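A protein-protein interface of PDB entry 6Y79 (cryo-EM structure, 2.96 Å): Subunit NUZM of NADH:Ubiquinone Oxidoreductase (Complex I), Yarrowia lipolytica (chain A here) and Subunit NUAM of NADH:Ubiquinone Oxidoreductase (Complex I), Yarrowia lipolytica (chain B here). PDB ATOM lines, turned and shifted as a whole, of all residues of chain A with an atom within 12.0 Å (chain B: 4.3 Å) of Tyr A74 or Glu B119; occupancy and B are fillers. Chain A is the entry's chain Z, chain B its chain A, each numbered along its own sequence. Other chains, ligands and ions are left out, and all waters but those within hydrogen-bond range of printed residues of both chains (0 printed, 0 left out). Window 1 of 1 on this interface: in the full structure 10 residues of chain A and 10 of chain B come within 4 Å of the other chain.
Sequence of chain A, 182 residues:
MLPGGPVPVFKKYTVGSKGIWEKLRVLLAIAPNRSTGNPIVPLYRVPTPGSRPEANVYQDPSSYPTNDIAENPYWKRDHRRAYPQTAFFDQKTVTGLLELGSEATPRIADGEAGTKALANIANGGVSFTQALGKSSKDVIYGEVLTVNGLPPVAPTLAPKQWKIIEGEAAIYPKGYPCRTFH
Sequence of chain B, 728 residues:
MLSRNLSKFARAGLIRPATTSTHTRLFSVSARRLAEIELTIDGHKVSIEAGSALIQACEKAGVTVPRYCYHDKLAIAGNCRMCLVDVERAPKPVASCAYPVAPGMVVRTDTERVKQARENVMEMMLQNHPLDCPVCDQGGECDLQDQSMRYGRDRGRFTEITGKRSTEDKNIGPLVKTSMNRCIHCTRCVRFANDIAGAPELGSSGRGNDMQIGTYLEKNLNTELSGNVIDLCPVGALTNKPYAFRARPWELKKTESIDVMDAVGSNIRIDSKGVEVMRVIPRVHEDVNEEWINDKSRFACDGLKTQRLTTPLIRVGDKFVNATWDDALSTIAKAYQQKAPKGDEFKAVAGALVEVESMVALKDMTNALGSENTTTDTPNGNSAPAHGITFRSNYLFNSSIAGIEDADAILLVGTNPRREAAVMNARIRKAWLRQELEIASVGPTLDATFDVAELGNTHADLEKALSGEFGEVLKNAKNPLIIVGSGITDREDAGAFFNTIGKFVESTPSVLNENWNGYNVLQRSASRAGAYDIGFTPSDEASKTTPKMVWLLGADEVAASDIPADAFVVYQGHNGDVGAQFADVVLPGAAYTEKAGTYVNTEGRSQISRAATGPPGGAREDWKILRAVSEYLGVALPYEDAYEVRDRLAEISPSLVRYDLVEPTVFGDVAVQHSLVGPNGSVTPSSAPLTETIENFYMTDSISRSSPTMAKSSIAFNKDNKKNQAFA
Pro A73 touches Gln B116 (CB to OE1, 3.3 Å). Pro A73 touches Glu B119 (CB to OE1, 3.3 Å). Asp B154 touches Tyr A74. CB of Trp A75 touches CE of Lys B115 (3.7 Å).
OE1 of Glu B119 sits at hydrogen-bond distance from N of Tyr A74 (3.5 Å). The side-chain amide oxygen (OE1) of Gln B116 is in hydrogen-bond range of the indole nitrogen (NE1) of Trp A75 (2.9 Å). OE2 of Glu B119 lies within hydrogen-bond range of N of Trp A75, at 3.1 Å. OD2 of Asp B154 lies within salt-bridge range of NH1 of Arg A77, at 3.2 Å.
Of the 20 printed residues of chain A, 4 touch a printed residue of chain B.
The guanidinium group (NE) of Arg A77 sits close to the side-chain amide nitrogen (ND2) of Asn A72 (3.2 Å). O of Gln B116 lies within hydrogen-bond range of ND2 of Asn B120, at 2.8 Å. OH of Tyr A74 sits at hydrogen-bond distance from OD2 of Asp A78 (3.1 Å).
Printed residues of chain B within 4 Å of Tyr A74: Glu B119 (3.5 Å) and Asp B154 (3.6 Å). Of chain A, only Pro A73 (3.3 Å), Tyr A74 (3.5 Å) and Trp A75 (3.1 Å) come within 4 Å of Glu B119. Of chain A, only Pro A73 (3.3 Å) and Trp A75 (2.9 Å) come within 4 Å of Gln B116. No residue of chain A comes within 4 Å of Ala B117. No residue of chain A comes within 4 Å of Met B122. No residue of chain A comes within 4 Å of Glu B123. Of chain A, only Tyr A74 (3.6 Å) and Arg A77 (3.2 Å) come within 4 Å of Asp B154. Printed residues of chain B within 4 Å of Pro A73: Gln B116 and Glu B119. Printed residues of chain B within 4 Å of Trp A75: Lys B115 (3.7 Å), Gln B116 (2.9 Å) and Glu B119 (3.1 Å). Printed residues of chain B within 4 Å of Arg A77: Asp B154 (3.2 Å). Asp A68 touches none of the printed residues of chain B.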
ATOM      1  N   TYR A  64      17.280  16.569  16.463  1.00  0.00           N
ATOM      2  CA  TYR A  64      16.403  15.631  15.759  1.00  0.00           C
ATOM      3  C   TYR A  64      17.133  14.585  14.916  1.00  0.00           C
ATOM      4  O   TYR A  64      16.844  13.390  15.099  1.00  0.00           O
ATOM      5  CB  TYR A  64      15.349  16.361  14.923  1.00  0.00           C
ATOM      6  CG  TYR A  64      14.579  15.358  14.083  1.00  0.00           C
ATOM      7  CD1 TYR A  64      13.746  14.419  14.689  1.00  0.00           C
ATOM      8  CD2 TYR A  64      14.715  15.316  12.696  1.00  0.00           C
ATOM      9  CE1 TYR A  64      13.059  13.483  13.941  1.00  0.00           C
ATOM     10  CE2 TYR A  64      14.030  14.380  11.940  1.00  0.00           C
ATOM     11  CZ  TYR A  64      13.202  13.469  12.567  1.00  0.00           C
ATOM     12  OH  TYR A  64      12.515  12.539  11.819  1.00  0.00           O
ATOM     13  N   PRO A  65      18.047  14.914  13.987  1.00  0.00           N
ATOM     14  CA  PRO A  65      18.627  13.829  13.179  1.00  0.00           C
ATOM     15  C   PRO A  65      19.639  12.970  13.925  1.00  0.00           C
ATOM     16  O   PRO A  65      20.291  12.129  13.297  1.00  0.00           O
ATOM     17  CB  PRO A  65      19.294  14.572  12.007  1.00  0.00           C
ATOM     18  CG  PRO A  65      18.825  15.974  12.099  1.00  0.00           C
ATOM     19  CD  PRO A  65      18.627  16.199  13.550  1.00  0.00           C
ATOM     20  N   THR A  66      19.796  13.150  15.232  1.00  0.00           N
ATOM     21  CA  THR A  66      20.608  12.286  16.069  1.00  0.00           C
ATOM     22  C   THR A  66      19.793  11.438  17.026  1.00  0.00           C
ATOM     23  O   THR A  66      20.002  10.226  17.091  1.00  0.00           O
ATOM     24  CB  THR A  66      21.600  13.118  16.872  1.00  0.00           C
ATOM     25  OG1 THR A  66      22.325  13.971  15.980  1.00  0.00           O
ATOM     26  CG2 THR A  66      22.549  12.194  17.580  1.00  0.00           C
ATOM     27  N   ASN A  67      18.825  12.022  17.739  1.00  0.00           N
ATOM     28  CA  ASN A  67      17.993  11.201  18.610  1.00  0.00           C
ATOM     29  C   ASN A  67      17.009  10.335  17.845  1.00  0.00           C
ATOM     30  O   ASN A  67      16.302   9.544  18.479  1.00  0.00           O
ATOM     31  CB  ASN A  67      17.210  12.053  19.618  1.00  0.00           C
ATOM     32  CG  ASN A  67      16.120  12.950  18.980  1.00  0.00           C
ATOM     33  OD1 ASN A  67      15.991  13.085  17.770  1.00  0.00           O
ATOM     34  ND2 ASN A  67      15.313  13.554  19.840  1.00  0.00           N
ATOM     35  N   ASP A  68      16.912  10.552  16.531  1.00  0.00           N
ATOM     36  CA  ASP A  68      15.996   9.852  15.651  1.00  0.00           C
ATOM     37  C   ASP A  68      16.167   8.353  15.779  1.00  0.00           C
ATOM     38  O   ASP A  68      17.284   7.831  15.744  1.00  0.00           O
ATOM     39  CB  ASP A  68      16.239  10.285  14.208  1.00  0.00           C
ATOM     40  CG  ASP A  68      15.074   9.969  13.312  1.00  0.00           C
ATOM     41  OD1 ASP A  68      14.063   9.477  13.835  1.00  0.00           O
ATOM     42  OD2 ASP A  68      15.175  10.202  12.092  1.00  0.00           O
ATOM     43  N   ILE A  69      15.046   7.671  15.958  1.00  0.00           N
ATOM     44  CA  ILE A  69      15.125   6.285  16.373  1.00  0.00           C
ATOM     45  C   ILE A  69      15.454   5.380  15.193  1.00  0.00           C
ATOM     46  O   ILE A  69      16.239   4.441  15.333  1.00  0.00           O
ATOM     47  CB  ILE A  69      13.832   5.882  17.111  1.00  0.00           C
ATOM     48  CG1 ILE A  69      14.015   4.551  17.810  1.00  0.00           C
ATOM     49  CG2 ILE A  69      12.585   5.883  16.221  1.00  0.00           C
ATOM     50  CD1 ILE A  69      12.902   4.249  18.729  1.00  0.00           C
ATOM     51  N   ALA A  70      14.969   5.689  13.997  1.00  0.00           N
ATOM     52  CA  ALA A  70      14.945   4.670  12.962  1.00  0.00           C
ATOM     53  C   ALA A  70      15.786   4.968  11.728  1.00  0.00           C
ATOM     54  O   ALA A  70      16.382   4.038  11.182  1.00  0.00           O
ATOM     55  CB  ALA A  70      13.496   4.410  12.524  1.00  0.00           C
ATOM     56  N   GLU A  71      15.872   6.218  11.271  1.00  0.00           N
ATOM     57  CA  GLU A  71      16.504   6.464   9.974  1.00  0.00           C
ATOM     58  C   GLU A  71      17.996   6.730  10.025  1.00  0.00           C
ATOM     59  O   GLU A  71      18.653   6.549   8.999  1.00  0.00           O
ATOM     60  CB  GLU A  71      15.789   7.604   9.247  1.00  0.00           C
ATOM     61  CG  GLU A  71      14.516   7.116   8.619  1.00  0.00           C
ATOM     62  CD  GLU A  71      13.691   8.185   7.966  1.00  0.00           C
ATOM     63  OE1 GLU A  71      14.125   9.346   7.935  1.00  0.00           O
ATOM     64  OE2 GLU A  71      12.550   7.863   7.570  1.00  0.00           O
ATOM     65  N   ASN A  72      18.544   7.145  11.167  1.00  0.00           N
ATOM     66  CA  ASN A  72      19.981   7.318  11.003  1.00  0.00           C
ATOM     67  C   ASN A  72      20.737   6.056  11.404  1.00  0.00           C
ATOM     68  O   ASN A  72      20.383   5.397  12.384  1.00  0.00           O
ATOM     69  CB  ASN A  72      20.525   8.513  11.807  1.00  0.00           C
ATOM     70  CG  ASN A  72      20.110   8.521  13.277  1.00  0.00           C
ATOM     71  OD1 ASN A  72      19.395   7.642  13.755  1.00  0.00           O
ATOM     72  ND2 ASN A  72      20.595   9.511  14.007  1.00  0.00           N
ATOM     73  N   PRO A  73      21.724   5.642  10.617  1.00  0.00           N
ATOM     74  CA  PRO A  73      22.756   4.755  11.154  1.00  0.00           C
ATOM     75  C   PRO A  73      23.959   5.563  11.601  1.00  0.00           C
ATOM     76  O   PRO A  73      24.167   6.680  11.122  1.00  0.00           O
ATOM     77  CB  PRO A  73      23.067   3.840   9.973  1.00  0.00           C
ATOM     78  CG  PRO A  73      22.826   4.692   8.794  1.00  0.00           C
ATOM     79  CD  PRO A  73      21.774   5.703   9.147  1.00  0.00           C
ATOM     80  N   TYR A  74      24.748   5.018  12.525  1.00  0.00           N
ATOM     81  CA  TYR A  74      25.810   5.803  13.137  1.00  0.00           C
ATOM     82  C   TYR A  74      26.951   6.083  12.167  1.00  0.00           C
ATOM     83  O   TYR A  74      27.630   7.108  12.290  1.00  0.00           O
ATOM     84  CB  TYR A  74      26.331   5.096  14.386  1.00  0.00           C
ATOM     85  CG  TYR A  74      27.396   5.884  15.083  1.00  0.00           C
ATOM     86  CD1 TYR A  74      27.085   7.061  15.728  1.00  0.00           C
ATOM     87  CD2 TYR A  74      28.717   5.480  15.056  1.00  0.00           C
ATOM     88  CE1 TYR A  74      28.045   7.799  16.346  1.00  0.00           C
ATOM     89  CE2 TYR A  74      29.690   6.217  15.677  1.00  0.00           C
ATOM     90  CZ  TYR A  74      29.344   7.379  16.322  1.00  0.00           C
ATOM     91  OH  TYR A  74      30.300   8.135  16.952  1.00  0.00           O
ATOM     92  N   TRP A  75      27.157   5.214  11.177  1.00  0.00           N
ATOM     93  CA  TRP A  75      28.281   5.381  10.262  1.00  0.00           C
ATOM     94  C   TRP A  75      28.094   6.555   9.312  1.00  0.00           C
ATOM     95  O   TRP A  75      29.062   6.975   8.672  1.00  0.00           O
ATOM     96  CB  TRP A  75      28.509   4.096   9.467  1.00  0.00           C
ATOM     97  CG  TRP A  75      27.352   3.714   8.615  1.00  0.00           C
ATOM     98  CD1 TRP A  75      26.328   2.893   8.958  1.00  0.00           C
ATOM     99  CD2 TRP A  75      27.097   4.132   7.271  1.00  0.00           C
ATOM    100  NE1 TRP A  75      25.451   2.772   7.915  1.00  0.00           N
ATOM    101  CE2 TRP A  75      25.898   3.532   6.871  1.00  0.00           C
ATOM    102  CE3 TRP A  75      27.769   4.963   6.371  1.00  0.00           C
ATOM    103  CZ2 TRP A  75      25.355   3.731   5.613  1.00  0.00           C
ATOM    104  CZ3 TRP A  75      27.227   5.161   5.127  1.00  0.00           C
ATOM    105  CH2 TRP A  75      26.029   4.552   4.760  1.00  0.00           C
ATOM    106  N   LYS A  76      26.872   7.075   9.188  1.00  0.00           N
ATOM    107  CA  LYS A  76      26.630   8.265   8.384  1.00  0.00           C
ATOM    108  C   LYS A  76      26.913   9.544   9.152  1.00  0.00           C
ATOM    109  O   LYS A  76      27.268  10.560   8.547  1.00  0.00           O
ATOM    110  CB  LYS A  76      25.187   8.285   7.898  1.00  0.00           C
ATOM    111  CG  LYS A  76      24.855   7.202   6.914  1.00  0.00           C
ATOM    112  CD  LYS A  76      23.472   7.402   6.342  1.00  0.00           C
ATOM    113  CE  LYS A  76      23.472   8.518   5.332  1.00  0.00           C
ATOM    114  NZ  LYS A  76      24.253   8.126   4.134  1.00  0.00           N
ATOM    115  N   ARG A  77      26.758   9.522  10.473  1.00  0.00           N
ATOM    116  CA  ARG A  77      27.008  10.694  11.300  1.00  0.00           C
ATOM    117  C   ARG A  77      28.211  10.526  12.212  1.00  0.00           C
ATOM    118  O   ARG A  77      28.385  11.321  13.140  1.00  0.00           O
ATOM    119  CB  ARG A  77      25.776  11.034  12.134  1.00  0.00           C
ATOM    120  CG  ARG A  77      25.334   9.953  13.069  1.00  0.00           C
ATOM    121  CD  ARG A  77      24.131  10.404  13.857  1.00  0.00           C
ATOM    122  NE  ARG A  77      23.688   9.382  14.789  1.00  0.00           N
ATOM    123  CZ  ARG A  77      24.179   9.228  16.011  1.00  0.00           C
ATOM    124  NH1 ARG A  77      23.715   8.265  16.790  1.00  0.00           N
ATOM    125  NH2 ARG A  77      25.130  10.036  16.454  1.00  0.00           N
ATOM    126  N   ASP A  78      29.034   9.510  11.995  1.00  0.00           N
ATOM    127  CA  ASP A  78      30.329   9.475  12.645  1.00  0.00           C
ATOM    128  C   ASP A  78      31.292  10.371  11.889  1.00  0.00           C
ATOM    129  O   ASP A  78      31.315  10.382  10.657  1.00  0.00           O
ATOM    130  CB  ASP A  78      30.885   8.056  12.702  1.00  0.00           C
ATOM    131  CG  ASP A  78      32.222   7.993  13.401  1.00  0.00           C
ATOM    132  OD1 ASP A  78      33.245   8.163  12.720  1.00  0.00           O
ATOM    133  OD2 ASP A  78      32.260   7.786  14.631  1.00  0.00           O
ATOM    134  N   HIS A  79      32.088  11.124  12.632  1.00  0.00           N
ATOM    135  CA  HIS A  79      33.117  11.938  12.027  1.00  0.00           C
ATOM    136  C   HIS A  79      34.455  11.790  12.722  1.00  0.00           C
ATOM    137  O   HIS A  79      35.432  12.392  12.274  1.00  0.00           O
ATOM    138  CB  HIS A  79      32.692  13.410  12.010  1.00  0.00           C
ATOM    139  CG  HIS A  79      31.489  13.679  11.165  1.00  0.00           C
ATOM    140  ND1 HIS A  79      31.484  13.484   9.802  1.00  0.00           N
ATOM    141  CD2 HIS A  79      30.257  14.133  11.487  1.00  0.00           C
ATOM    142  CE1 HIS A  79      30.296  13.799   9.320  1.00  0.00           C
ATOM    143  NE2 HIS A  79      29.532  14.196  10.322  1.00  0.00           N
ATOM    144  N   ARG A  80      34.529  11.005  13.794  1.00  0.00           N
ATOM    145  CA  ARG A  80      35.826  10.681  14.372  1.00  0.00           C
ATOM    146  C   ARG A  80      36.586   9.704  13.487  1.00  0.00           C
ATOM    147  O   ARG A  80      37.808   9.805  13.357  1.00  0.00           O
ATOM    148  CB  ARG A  80      35.654  10.118  15.781  1.00  0.00           C
ATOM    149  CG  ARG A  80      36.955   9.895  16.510  1.00  0.00           C
ATOM    150  CD  ARG A  80      36.736   9.266  17.858  1.00  0.00           C
ATOM    151  NE  ARG A  80      36.226   7.909  17.764  1.00  0.00           N
ATOM    152  CZ  ARG A  80      35.966   7.148  18.817  1.00  0.00           C
ATOM    153  NH1 ARG A  80      35.502   5.927  18.651  1.00  0.00           N
ATOM    154  NH2 ARG A  80      36.170   7.616  20.034  1.00  0.00           N
ATOM    155  N   ARG A  81      35.888   8.761  12.858  1.00  0.00           N
ATOM    156  CA  ARG A  81      36.548   7.843  11.942  1.00  0.00           C
ATOM    157  C   ARG A  81      36.624   8.380  10.520  1.00  0.00           C
ATOM    158  O   ARG A  81      37.201   7.714   9.655  1.00  0.00           O
ATOM    159  CB  ARG A  81      35.841   6.485  11.937  1.00  0.00           C
ATOM    160  CG  ARG A  81      35.894   5.782  13.270  1.00  0.00           C
ATOM    161  CD  ARG A  81      34.976   4.588  13.325  1.00  0.00           C
ATOM    162  NE  ARG A  81      35.075   3.930  14.622  1.00  0.00           N
ATOM    163  CZ  ARG A  81      34.243   4.137  15.633  1.00  0.00           C
ATOM    164  NH1 ARG A  81      33.236   4.975  15.494  1.00  0.00           N
ATOM    165  NH2 ARG A  81      34.420   3.500  16.780  1.00  0.00           N
ATOM    166  N   ALA A  82      36.064   9.559  10.258  1.00  0.00           N
ATOM    167  CA  ALA A  82      36.193  10.226   8.970  1.00  0.00           C
ATOM    168  C   ALA A  82      37.197  11.371   9.014  1.00  0.00           C
ATOM    169  O   ALA A  82      37.035  12.366   8.303  1.00  0.00           O
ATOM    170  CB  ALA A  82      34.833  10.732   8.497  1.00  0.00           C
ATOM    171  N   TYR A  83      38.227  11.249   9.842  1.00  0.00           N
ATOM    172  CA  TYR A  83      39.262  12.263   9.935  1.00  0.00           C
ATOM    173  C   TYR A  83      40.114  12.282   8.666  1.00  0.00           C
ATOM    174  O   TYR A  83      40.313  11.248   8.031  1.00  0.00           O
ATOM    175  CB  TYR A  83      40.152  12.003  11.150  1.00  0.00           C
ATOM    176  CG  TYR A  83      40.947  10.705  11.127  1.00  0.00           C
ATOM    177  CD1 TYR A  83      40.353   9.501  11.473  1.00  0.00           C
ATOM    178  CD2 TYR A  83      42.296  10.693  10.801  1.00  0.00           C
ATOM    179  CE1 TYR A  83      41.060   8.329  11.470  1.00  0.00           C
ATOM    180  CE2 TYR A  83      43.015   9.517  10.797  1.00  0.00           C
ATOM    181  CZ  TYR A  83      42.389   8.338  11.135  1.00  0.00           C
ATOM    182  OH  TYR A  83      43.092   7.157  11.138  1.00  0.00           O
ATOM    183  N   LYS B 115      29.066  -1.741   6.228  1.00  0.00           N
ATOM    184  CA  LYS B 115      28.989  -1.038   7.508  1.00  0.00           C
ATOM    185  C   LYS B 115      27.565  -1.059   8.066  1.00  0.00           C
ATOM    186  O   LYS B 115      27.366  -1.249   9.280  1.00  0.00           O
ATOM    187  CB  LYS B 115      29.496   0.394   7.340  1.00  0.00           C
ATOM    188  CG  LYS B 115      30.973   0.476   6.959  1.00  0.00           C
ATOM    189  CD  LYS B 115      31.395   1.907   6.651  1.00  0.00           C
ATOM    190  CE  LYS B 115      31.544   2.731   7.910  1.00  0.00           C
ATOM    191  NZ  LYS B 115      31.904   4.148   7.629  1.00  0.00           N
ATOM    192  N   GLN B 116      26.567  -0.939   7.181  1.00  0.00           N
ATOM    193  CA  GLN B 116      25.173  -1.079   7.592  1.00  0.00           C
ATOM    194  C   GLN B 116      24.878  -2.483   8.102  1.00  0.00           C
ATOM    195  O   GLN B 116      24.184  -2.645   9.110  1.00  0.00           O
ATOM    196  CB  GLN B 116      24.250  -0.733   6.424  1.00  0.00           C
ATOM    197  CG  GLN B 116      22.778  -0.771   6.767  1.00  0.00           C
ATOM    198  CD  GLN B 116      22.401   0.297   7.758  1.00  0.00           C
ATOM    199  OE1 GLN B 116      22.861   1.431   7.664  1.00  0.00           O
ATOM    200  NE2 GLN B 116      21.570  -0.059   8.726  1.00  0.00           N
ATOM    201  N   ALA B 117      25.431  -3.506   7.442  1.00  0.00           N
ATOM    202  CA  ALA B 117      25.200  -4.886   7.859  1.00  0.00           C
ATOM    203  C   ALA B 117      25.831  -5.174   9.214  1.00  0.00           C
ATOM    204  O   ALA B 117      25.249  -5.894  10.036  1.00  0.00           O
ATOM    205  CB  ALA B 117      25.749  -5.843   6.805  1.00  0.00           C
ATOM    206  N   ARG B 118      27.012  -4.607   9.469  1.00  0.00           N
ATOM    207  CA  ARG B 118      27.670  -4.822  10.752  1.00  0.00           C
ATOM    208  C   ARG B 118      26.912  -4.145  11.884  1.00  0.00           C
ATOM    209  O   ARG B 118      26.759  -4.729  12.965  1.00  0.00           O
ATOM    210  CB  ARG B 118      29.115  -4.338  10.680  1.00  0.00           C
ATOM    211  CG  ARG B 118      29.941  -5.226   9.787  1.00  0.00           C
ATOM    212  CD  ARG B 118      31.360  -4.770   9.605  1.00  0.00           C
ATOM    213  NE  ARG B 118      32.033  -5.678   8.684  1.00  0.00           N
ATOM    214  CZ  ARG B 118      33.291  -5.557   8.291  1.00  0.00           C
ATOM    215  NH1 ARG B 118      34.035  -4.562   8.748  1.00  0.00           N
ATOM    216  NH2 ARG B 118      33.807  -6.439   7.449  1.00  0.00           N
ATOM    217  N   GLU B 119      26.373  -2.946  11.631  1.00  0.00           N
ATOM    218  CA  GLU B 119      25.552  -2.296  12.650  1.00  0.00           C
ATOM    219  C   GLU B 119      24.250  -3.046  12.891  1.00  0.00           C
ATOM    220  O   GLU B 119      23.796  -3.158  14.040  1.00  0.00           O
ATOM    221  CB  GLU B 119      25.259  -0.861  12.257  1.00  0.00           C
ATOM    222  CG  GLU B 119      26.478  -0.001  12.289  1.00  0.00           C
ATOM    223  CD  GLU B 119      26.164   1.415  11.952  1.00  0.00           C
ATOM    224  OE1 GLU B 119      25.004   1.678  11.587  1.00  0.00           O
ATOM    225  OE2 GLU B 119      27.069   2.269  12.034  1.00  0.00           O
ATOM    226  N   ASN B 120      23.653  -3.585  11.823  1.00  0.00           N
ATOM    227  CA  ASN B 120      22.422  -4.359  11.949  1.00  0.00           C
ATOM    228  C   ASN B 120      22.636  -5.601  12.802  1.00  0.00           C
ATOM    229  O   ASN B 120      21.940  -5.800  13.800  1.00  0.00           O
ATOM    230  CB  ASN B 120      21.900  -4.747  10.567  1.00  0.00           C
ATOM    231  CG  ASN B 120      21.356  -3.567   9.795  1.00  0.00           C
ATOM    232  OD1 ASN B 120      20.673  -2.705  10.344  1.00  0.00           O
ATOM    233  ND2 ASN B 120      21.648  -3.531   8.503  1.00  0.00           N
ATOM    234  N   VAL B 121      23.638  -6.415  12.452  1.00  0.00           N
ATOM    235  CA  VAL B 121      23.900  -7.662  13.172  1.00  0.00           C
ATOM    236  C   VAL B 121      24.350  -7.394  14.610  1.00  0.00           C
ATOM    237  O   VAL B 121      23.985  -8.144  15.531  1.00  0.00           O
ATOM    238  CB  VAL B 121      24.920  -8.506  12.373  1.00  0.00           C
ATOM    239  CG1 VAL B 121      25.338  -9.762  13.120  1.00  0.00           C
ATOM    240  CG2 VAL B 121      24.334  -8.891  11.022  1.00  0.00           C
ATOM    241  N   MET B 122      25.066  -6.286  14.845  1.00  0.00           N
ATOM    242  CA  MET B 122      25.431  -5.922  16.214  1.00  0.00           C
ATOM    243  C   MET B 122      24.212  -5.564  17.055  1.00  0.00           C
ATOM    244  O   MET B 122      24.091  -6.021  18.203  1.00  0.00           O
ATOM    245  CB  MET B 122      26.397  -4.747  16.205  1.00  0.00           C
ATOM    246  CG  MET B 122      26.945  -4.437  17.570  1.00  0.00           C
ATOM    247  SD  MET B 122      27.948  -5.823  18.089  1.00  0.00           S
ATOM    248  CE  MET B 122      29.271  -5.636  16.911  1.00  0.00           C
ATOM    249  N   GLU B 123      23.303  -4.749  16.500  1.00  0.00           N
ATOM    250  CA  GLU B 123      22.089  -4.380  17.223  1.00  0.00           C
ATOM    251  C   GLU B 123      21.219  -5.598  17.491  1.00  0.00           C
ATOM    252  O   GLU B 123      20.571  -5.698  18.540  1.00  0.00           O
ATOM    253  CB  GLU B 123      21.305  -3.337  16.432  1.00  0.00           C
ATOM    254  CG  GLU B 123      20.071  -2.829  17.160  1.00  0.00           C
ATOM    255  CD  GLU B 123      19.295  -1.803  16.374  1.00  0.00           C
ATOM    256  OE1 GLU B 123      19.704  -1.476  15.243  1.00  0.00           O
ATOM    257  OE2 GLU B 123      18.263  -1.327  16.888  1.00  0.00           O
ATOM    258  N   TYR B 151      32.271  -1.130  15.481  1.00  0.00           N
ATOM    259  CA  TYR B 151      31.405  -1.466  14.365  1.00  0.00           C
ATOM    260  C   TYR B 151      29.924  -1.288  14.630  1.00  0.00           C
ATOM    261  O   TYR B 151      29.153  -1.254  13.668  1.00  0.00           O
ATOM    262  CB  TYR B 151      31.647  -2.915  13.923  1.00  0.00           C
ATOM    263  CG  TYR B 151      33.021  -3.099  13.355  1.00  0.00           C
ATOM    264  CD1 TYR B 151      33.321  -2.630  12.090  1.00  0.00           C
ATOM    265  CD2 TYR B 151      34.021  -3.727  14.079  1.00  0.00           C
ATOM    266  CE1 TYR B 151      34.574  -2.775  11.561  1.00  0.00           C
ATOM    267  CE2 TYR B 151      35.282  -3.888  13.552  1.00  0.00           C
ATOM    268  CZ  TYR B 151      35.554  -3.401  12.295  1.00  0.00           C
ATOM    269  OH  TYR B 151      36.810  -3.552  11.763  1.00  0.00           O
ATOM    270  N   GLY B 152      29.502  -1.171  15.885  1.00  0.00           N
ATOM    271  CA  GLY B 152      28.097  -1.216  16.208  1.00  0.00           C
ATOM    272  C   GLY B 152      27.439   0.148  16.248  1.00  0.00           C
ATOM    273  O   GLY B 152      28.043   1.185  15.977  1.00  0.00           O
ATOM    274  N   ASP B 154      25.538   3.405  17.952  1.00  0.00           N
ATOM    275  CA  ASP B 154      25.654   4.297  19.100  1.00  0.00           C
ATOM    276  C   ASP B 154      24.655   3.920  20.187  1.00  0.00           C
ATOM    277  O   ASP B 154      25.041   3.495  21.279  1.00  0.00           O
ATOM    278  CB  ASP B 154      25.406   5.738  18.643  1.00  0.00           C
ATOM    279  CG  ASP B 154      25.760   6.777  19.687  1.00  0.00           C
ATOM    280  OD1 ASP B 154      26.248   6.421  20.777  1.00  0.00           O
ATOM    281  OD2 ASP B 154      25.536   7.973  19.409  1.00  0.00           O
